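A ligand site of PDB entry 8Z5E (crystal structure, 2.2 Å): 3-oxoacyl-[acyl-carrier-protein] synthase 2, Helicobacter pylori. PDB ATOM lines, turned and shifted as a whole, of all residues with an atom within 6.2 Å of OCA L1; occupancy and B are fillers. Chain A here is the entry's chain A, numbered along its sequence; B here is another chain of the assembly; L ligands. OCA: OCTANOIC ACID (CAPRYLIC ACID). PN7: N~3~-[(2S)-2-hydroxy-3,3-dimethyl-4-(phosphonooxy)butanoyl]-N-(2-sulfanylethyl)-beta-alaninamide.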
ATOM      1  N   GLY A 112      23.406   5.871  24.234  1.00  0.00           N
ATOM      2  CA  GLY A 112      24.359   5.736  25.354  1.00  0.00           C
ATOM      3  C   GLY A 112      25.758   6.227  24.998  1.00  0.00           C
ATOM      4  O   GLY A 112      26.344   6.958  25.814  1.00  0.00           O
ATOM      5  N   ILE A 113      26.269   5.867  23.817  1.00  0.00           N
ATOM      6  CA  ILE A 113      27.680   6.229  23.454  1.00  0.00           C
ATOM      7  C   ILE A 113      27.764   6.640  21.978  1.00  0.00           C
ATOM      8  O   ILE A 113      28.766   7.282  21.610  1.00  0.00           O
ATOM      9  CB  ILE A 113      28.628   5.062  23.775  1.00  0.00           C
ATOM     10  CG1 ILE A 113      30.071   5.551  23.970  1.00  0.00           C
ATOM     11  CG2 ILE A 113      28.535   3.972  22.709  1.00  0.00           C
ATOM     12  CD1 ILE A 113      31.023   4.477  24.433  1.00  0.00           C
ATOM     13  N   LEU A 116      30.678   4.293  18.741  1.00  0.00           N
ATOM     14  CA  LEU A 116      31.838   3.705  19.469  1.00  0.00           C
ATOM     15  C   LEU A 116      32.809   3.072  18.462  1.00  0.00           C
ATOM     16  O   LEU A 116      34.018   3.303  18.598  1.00  0.00           O
ATOM     17  CB  LEU A 116      31.325   2.675  20.469  1.00  0.00           C
ATOM     18  CG  LEU A 116      32.403   1.920  21.247  1.00  0.00           C
ATOM     19  CD1 LEU A 116      33.243   2.890  22.064  1.00  0.00           C
ATOM     20  CD2 LEU A 116      31.775   0.870  22.146  1.00  0.00           C
ATOM     21  N   THR A 166      21.729   9.330  28.887  1.00  0.00           N
ATOM     22  CA  THR A 166      21.639   8.649  30.184  1.00  0.00           C
ATOM     23  C   THR A 166      21.690   7.135  30.041  1.00  0.00           C
ATOM     24  O   THR A 166      20.850   6.425  30.578  1.00  0.00           O
ATOM     25  CB  THR A 166      20.373   9.072  30.934  1.00  0.00           C
ATOM     26  OG1 THR A 166      19.348   9.395  29.998  1.00  0.00           O
ATOM     27  CG2 THR A 166      20.653  10.288  31.895  1.00  0.00           C
ATOM     28  N   ALA A 167      22.696   6.645  29.306  1.00  0.00           N
ATOM     29  CA  ALA A 167      23.059   5.252  29.337  1.00  0.00           C
ATOM     30  C   ALA A 167      21.866   4.406  28.939  1.00  0.00           C
ATOM     31  O   ALA A 167      21.202   4.718  27.957  1.00  0.00           O
ATOM     32  CB  ALA A 167      23.579   4.872  30.750  1.00  0.00           C
ATOM     33  N   CYS A 168      21.543   3.357  29.701  1.00  0.00           N
ATOM     34  CA  CYS A 168      20.478   2.403  29.271  1.00  0.00           C
ATOM     35  C   CYS A 168      19.074   3.010  29.502  1.00  0.00           C
ATOM     36  O   CYS A 168      18.090   2.359  29.133  1.00  0.00           O
ATOM     37  CB  CYS A 168      20.720   1.008  29.878  1.00  0.00           C
ATOM     38  SG  CYS A 168      22.253   0.265  29.290  1.00  0.00           S
ATOM     39  N   ALA A 169      19.014   4.222  30.048  1.00  0.00           N
ATOM     40  CA  ALA A 169      17.732   4.915  30.165  1.00  0.00           C
ATOM     41  C   ALA A 169      17.563   6.060  29.136  1.00  0.00           C
ATOM     42  O   ALA A 169      16.533   6.750  29.152  1.00  0.00           O
ATOM     43  CB  ALA A 169      17.551   5.461  31.604  1.00  0.00           C
ATOM     44  N   GLU A 196      20.994   2.777  18.955  1.00  0.00           N
ATOM     45  CA  GLU A 196      22.243   2.294  19.495  1.00  0.00           C
ATOM     46  C   GLU A 196      22.758   1.170  18.620  1.00  0.00           C
ATOM     47  O   GLU A 196      21.986   0.308  18.187  1.00  0.00           O
ATOM     48  CB  GLU A 196      22.083   1.815  20.947  1.00  0.00           C
ATOM     49  CG  GLU A 196      23.410   1.612  21.678  1.00  0.00           C
ATOM     50  CD  GLU A 196      23.825   2.820  22.524  1.00  0.00           C
ATOM     51  OE1 GLU A 196      23.066   3.169  23.462  1.00  0.00           O
ATOM     52  OE2 GLU A 196      24.883   3.441  22.226  1.00  0.00           O
ATOM     53  N   THR A 198      26.498  -0.865  19.007  1.00  0.00           N
ATOM     54  CA  THR A 198      27.823  -0.910  19.626  1.00  0.00           C
ATOM     55  C   THR A 198      28.404  -2.328  19.620  1.00  0.00           C
ATOM     56  O   THR A 198      29.197  -2.681  20.502  1.00  0.00           O
ATOM     57  CB  THR A 198      27.770  -0.391  21.061  1.00  0.00           C
ATOM     58  OG1 THR A 198      26.794  -1.149  21.793  1.00  0.00           O
ATOM     59  CG2 THR A 198      27.359   1.079  21.073  1.00  0.00           C
ATOM     60  N   GLY A 203      33.307  -2.415  22.523  1.00  0.00           N
ATOM     61  CA  GLY A 203      32.007  -2.408  23.162  1.00  0.00           C
ATOM     62  C   GLY A 203      31.675  -3.734  23.837  1.00  0.00           C
ATOM     63  O   GLY A 203      31.296  -3.766  25.001  1.00  0.00           O
ATOM     64  N   PHE A 207      31.827  -4.579  28.190  1.00  0.00           N
ATOM     65  CA  PHE A 207      30.820  -5.196  29.050  1.00  0.00           C
ATOM     66  C   PHE A 207      31.229  -6.582  29.530  1.00  0.00           C
ATOM     67  O   PHE A 207      30.806  -7.001  30.610  1.00  0.00           O
ATOM     68  CB  PHE A 207      29.483  -5.253  28.319  1.00  0.00           C
ATOM     69  CG  PHE A 207      28.740  -3.942  28.306  1.00  0.00           C
ATOM     70  CD1 PHE A 207      28.125  -3.482  29.452  1.00  0.00           C
ATOM     71  CD2 PHE A 207      28.668  -3.178  27.154  1.00  0.00           C
ATOM     72  CE1 PHE A 207      27.434  -2.280  29.440  1.00  0.00           C
ATOM     73  CE2 PHE A 207      27.990  -1.971  27.131  1.00  0.00           C
ATOM     74  CZ  PHE A 207      27.370  -1.521  28.285  1.00  0.00           C
ATOM     75  N   PHE A 234      23.320  -9.890  30.308  1.00  0.00           N
ATOM     76  CA  PHE A 234      22.470  -9.487  29.196  1.00  0.00           C
ATOM     77  C   PHE A 234      23.123  -9.869  27.875  1.00  0.00           C
ATOM     78  O   PHE A 234      24.268 -10.329  27.817  1.00  0.00           O
ATOM     79  CB  PHE A 234      22.098  -7.990  29.281  1.00  0.00           C
ATOM     80  CG  PHE A 234      23.181  -7.033  28.861  1.00  0.00           C
ATOM     81  CD1 PHE A 234      24.119  -6.577  29.775  1.00  0.00           C
ATOM     82  CD2 PHE A 234      23.204  -6.515  27.572  1.00  0.00           C
ATOM     83  CE1 PHE A 234      25.098  -5.652  29.406  1.00  0.00           C
ATOM     84  CE2 PHE A 234      24.163  -5.573  27.179  1.00  0.00           C
ATOM     85  CZ  PHE A 234      25.122  -5.145  28.104  1.00  0.00           C
ATOM     86  N   MET A 236      23.813  -8.073  24.169  1.00  0.00           N
ATOM     87  CA  MET A 236      23.783  -6.741  23.591  1.00  0.00           C
ATOM     88  C   MET A 236      23.013  -6.773  22.286  1.00  0.00           C
ATOM     89  O   MET A 236      23.242  -7.631  21.436  1.00  0.00           O
ATOM     90  CB  MET A 236      25.202  -6.205  23.376  1.00  0.00           C
ATOM     91  CG  MET A 236      25.268  -4.880  22.586  1.00  0.00           C
ATOM     92  SD  MET A 236      26.951  -4.414  22.121  1.00  0.00           S
ATOM     93  CE  MET A 236      27.692  -4.188  23.739  1.00  0.00           C
ATOM     94  N   HIS A 305      12.263  -3.147  32.235  1.00  0.00           N
ATOM     95  CA  HIS A 305      13.631  -2.986  31.754  1.00  0.00           C
ATOM     96  C   HIS A 305      14.249  -4.353  31.495  1.00  0.00           C
ATOM     97  O   HIS A 305      14.681  -4.655  30.379  1.00  0.00           O
ATOM     98  CB  HIS A 305      14.439  -2.172  32.771  1.00  0.00           C
ATOM     99  CG  HIS A 305      15.763  -1.722  32.243  1.00  0.00           C
ATOM    100  ND1 HIS A 305      15.899  -1.035  31.053  1.00  0.00           N
ATOM    101  CD2 HIS A 305      17.020  -1.854  32.740  1.00  0.00           C
ATOM    102  CE1 HIS A 305      17.175  -0.790  30.831  1.00  0.00           C
ATOM    103  NE2 HIS A 305      17.877  -1.265  31.847  1.00  0.00           N
ATOM    104  N   HIS A 342      19.044  -6.665  24.890  1.00  0.00           N
ATOM    105  CA  HIS A 342      18.907  -5.359  25.509  1.00  0.00           C
ATOM    106  C   HIS A 342      19.639  -4.337  24.650  1.00  0.00           C
ATOM    107  O   HIS A 342      20.842  -4.487  24.389  1.00  0.00           O
ATOM    108  CB  HIS A 342      19.432  -5.344  26.940  1.00  0.00           C
ATOM    109  CG  HIS A 342      19.548  -3.961  27.495  1.00  0.00           C
ATOM    110  ND1 HIS A 342      18.436  -3.163  27.711  1.00  0.00           N
ATOM    111  CD2 HIS A 342      20.622  -3.193  27.782  1.00  0.00           C
ATOM    112  CE1 HIS A 342      18.821  -1.978  28.155  1.00  0.00           C
ATOM    113  NE2 HIS A 342      20.141  -1.972  28.207  1.00  0.00           N
ATOM    114  N   LEU A 344      20.307  -1.067  25.057  1.00  0.00           N
ATOM    115  CA  LEU A 344      21.076   0.008  25.679  1.00  0.00           C
ATOM    116  C   LEU A 344      20.320   1.323  25.483  1.00  0.00           C
ATOM    117  O   LEU A 344      19.139   1.396  25.870  1.00  0.00           O
ATOM    118  CB  LEU A 344      22.502   0.002  25.135  1.00  0.00           C
ATOM    119  CG  LEU A 344      23.285  -1.304  25.194  1.00  0.00           C
ATOM    120  CD1 LEU A 344      24.451  -1.269  24.202  1.00  0.00           C
ATOM    121  CD2 LEU A 344      23.766  -1.561  26.617  1.00  0.00           C
ATOM    122  N   GLY A 345      20.935   2.359  24.913  1.00  0.00           N
ATOM    123  CA  GLY A 345      20.306   3.673  24.822  1.00  0.00           C
ATOM    124  C   GLY A 345      19.053   3.680  23.979  1.00  0.00           C
ATOM    125  O   GLY A 345      18.205   4.557  24.161  1.00  0.00           O
ATOM    126  N   PHE A 399      16.446   1.795  33.214  1.00  0.00           N
ATOM    127  CA  PHE A 399      17.472   2.172  34.191  1.00  0.00           C
ATOM    128  C   PHE A 399      18.849   2.101  33.538  1.00  0.00           C
ATOM    129  O   PHE A 399      19.099   1.268  32.659  1.00  0.00           O
ATOM    130  CB  PHE A 399      17.410   1.260  35.426  1.00  0.00           C
ATOM    131  CG  PHE A 399      16.009   0.853  35.799  1.00  0.00           C
ATOM    132  CD1 PHE A 399      15.062   1.804  36.156  1.00  0.00           C
ATOM    133  CD2 PHE A 399      15.639  -0.496  35.783  1.00  0.00           C
ATOM    134  CE1 PHE A 399      13.781   1.429  36.486  1.00  0.00           C
ATOM    135  CE2 PHE A 399      14.347  -0.887  36.112  1.00  0.00           C
ATOM    136  CZ  PHE A 399      13.415   0.090  36.462  1.00  0.00           C
ATOM    137  N   GLY A 400      19.751   2.982  33.996  1.00  0.00           N
ATOM    138  CA  GLY A 400      21.062   3.083  33.409  1.00  0.00           C
ATOM    139  C   GLY A 400      22.160   3.161  34.458  1.00  0.00           C
ATOM    140  O   GLY A 400      21.937   3.521  35.618  1.00  0.00           O
ATOM    141  N   PHE A 401      23.360   2.789  34.007  1.00  0.00           N
ATOM    142  CA  PHE A 401      24.564   3.026  34.805  1.00  0.00           C
ATOM    143  C   PHE A 401      24.567   4.451  35.344  1.00  0.00           C
ATOM    144  O   PHE A 401      24.090   5.390  34.700  1.00  0.00           O
ATOM    145  CB  PHE A 401      25.825   2.824  33.957  1.00  0.00           C
ATOM    146  CG  PHE A 401      26.183   1.389  33.722  1.00  0.00           C
ATOM    147  CD1 PHE A 401      25.443   0.363  34.303  1.00  0.00           C
ATOM    148  CD2 PHE A 401      27.269   1.070  32.917  1.00  0.00           C
ATOM    149  CE1 PHE A 401      25.781  -0.964  34.094  1.00  0.00           C
ATOM    150  CE2 PHE A 401      27.618  -0.250  32.687  1.00  0.00           C
ATOM    151  CZ  PHE A 401      26.858  -1.275  33.281  1.00  0.00           C
ATOM    152  N   ILE B 139      34.022   1.492  30.904  1.00  0.00           N
ATOM    153  CA  ILE B 139      32.733   2.052  30.479  1.00  0.00           C
ATOM    154  C   ILE B 139      32.285   3.186  31.397  1.00  0.00           C
ATOM    155  O   ILE B 139      31.987   4.300  30.938  1.00  0.00           O
ATOM    156  CB  ILE B 139      31.649   0.952  30.404  1.00  0.00           C
ATOM    157  CG1 ILE B 139      31.940  -0.003  29.257  1.00  0.00           C
ATOM    158  CG2 ILE B 139      30.270   1.583  30.234  1.00  0.00           C
ATOM    159  CD1 ILE B 139      30.902  -1.124  29.089  1.00  0.00           C
ATOM    160  N   LEU B 143      31.325   7.285  29.947  1.00  0.00           N
ATOM    161  CA  LEU B 143      29.999   7.722  29.543  1.00  0.00           C
ATOM    162  C   LEU B 143      29.723   9.121  30.067  1.00  0.00           C
ATOM    163  O   LEU B 143      29.978   9.422  31.226  1.00  0.00           O
ATOM    164  CB  LEU B 143      28.916   6.769  30.045  1.00  0.00           C
ATOM    165  CG  LEU B 143      28.968   5.271  29.740  1.00  0.00           C
ATOM    166  CD1 LEU B 143      27.890   4.559  30.570  1.00  0.00           C
ATOM    167  CD2 LEU B 143      28.801   5.014  28.268  1.00  0.00           C
ATOM    168  N   ASN B 145      26.995  10.577  30.947  1.00  0.00           N
ATOM    169  CA  ASN B 145      26.084  10.716  32.092  1.00  0.00           C
ATOM    170  C   ASN B 145      26.733  10.330  33.412  1.00  0.00           C
ATOM    171  O   ASN B 145      26.187  10.665  34.480  1.00  0.00           O
ATOM    172  CB  ASN B 145      24.815   9.888  31.905  1.00  0.00           C
ATOM    173  CG  ASN B 145      25.048   8.412  32.062  1.00  0.00           C
ATOM    174  OD1 ASN B 145      25.788   7.818  31.273  1.00  0.00           O
ATOM    175  ND2 ASN B 145      24.424   7.811  33.064  1.00  0.00           N
HETATM  176  C1  OCA L   1      23.397   0.776  30.545  1.00  0.00           C
HETATM  177  C2  OCA L   1      24.800   0.279  30.317  1.00  0.00           C
HETATM  178  C3  OCA L   1      25.717   1.378  29.849  1.00  0.00           C
HETATM  179  C4  OCA L   1      25.074   2.355  28.876  1.00  0.00           C
HETATM  180  C5  OCA L   1      25.419   2.125  27.416  1.00  0.00           C
HETATM  181  C6  OCA L   1      26.894   2.234  27.084  1.00  0.00           C
HETATM  182  C7  OCA L   1      27.304   1.680  25.733  1.00  0.00           C
HETATM  183  C8  OCA L   1      28.776   1.445  25.579  1.00  0.00           C
HETATM  184  O1  OCA L   1      23.073   1.446  31.495  1.00  0.00           O
HETATM  185  O3  PN7 L   2      26.586  -4.683  39.235  1.00  0.00           O
HETATM  186  O4  PN7 L   2      25.023  -6.179  36.995  1.00  0.00           O
HETATM  187  C2  PN7 L   2      27.929  -5.759  37.484  1.00  0.00           C
HETATM  188  C1  PN7 L   2      29.050  -5.573  38.500  1.00  0.00           C
HETATM  189  P   PN7 L   2      28.908  -6.012  41.093  1.00  0.00           P
HETATM  190  O1P PN7 L   2      28.301  -7.102  41.898  1.00  0.00           O
HETATM  191  O2P PN7 L   2      28.314  -4.641  41.164  1.00  0.00           O
HETATM  192  O3P PN7 L   2      28.916  -6.503  39.567  1.00  0.00           O
HETATM  193  CE1 PN7 L   2      28.428  -5.374  36.106  1.00  0.00           C
HETATM  194  CE2 PN7 L   2      27.500  -7.215  37.466  1.00  0.00           C
HETATM  195  C3  PN7 L   2      26.796  -4.766  37.825  1.00  0.00           C
HETATM  196  C4  PN7 L   2      25.479  -5.060  37.146  1.00  0.00           C
HETATM  197  N5  PN7 L   2      24.883  -3.945  36.762  1.00  0.00           N
HETATM  198  C6  PN7 L   2      23.661  -3.597  36.067  1.00  0.00           C
HETATM  199  C7  PN7 L   2      22.592  -4.667  36.192  1.00  0.00           C
HETATM  200  C8  PN7 L   2      21.525  -4.180  35.244  1.00  0.00           C
HETATM  201  O8  PN7 L   2      21.131  -4.873  34.325  1.00  0.00           O
HETATM  202  N9  PN7 L   2      21.094  -2.950  35.478  1.00  0.00           N
HETATM  203  C10 PN7 L   2      20.093  -2.190  34.741  1.00  0.00           C
HETATM  204  C11 PN7 L   2      20.809  -0.930  34.274  1.00  0.00           C
HETATM  205  S12 PN7 L   2      22.160  -1.374  33.177  1.00  0.00           S
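SG of Cys 168 is covalently linked to C1 of OCA L1, 1.8 Å away.
The backbone NH (N) of Phe 401 lies within hydrogen-bond range of an oxygen (O1) of OCA L1.
The backbone NH (N) of Cys 168 lies close to an oxygen (O1) of OCA L1 (3.0 Å).
S12 of PN7 L2 sits close to O1 of OCA L1.
The side-chain amide nitrogen (ND2) of Asn 145 of chain B is in hydrogen-bond range of the backbone carbonyl oxygen (O) of Phe 401, at 2.9 Å.
The side-chain carboxylate (OE2) of Glu 196 lies within hydrogen-bond range of the backbone NH (N) of Ile 113 (3.2 Å).
The side-chain sulfur of Cys 168 sits at hydrogen-bond distance from a ring nitrogen (NE2) of His 342 (3.3 Å).
Ile 113 touches OCA L1.
CB of Ala 167 touches C4 of OCA L1 (3.5 Å).
CZ of Phe 207 touches C3 of OCA L1, at 3.7 Å.
CA of Gly 400 touches O1 of OCA L1, 3.2 Å away.
Leu 143 of chain B touches OCA L1 (CD2 to C6, 3.6 Å).
Hydrophobic or aromatic side chains within 4 Å of OCA L1: Ile 113, Ala 167, Phe 207, Phe 401 and Leu 143 of chain B.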
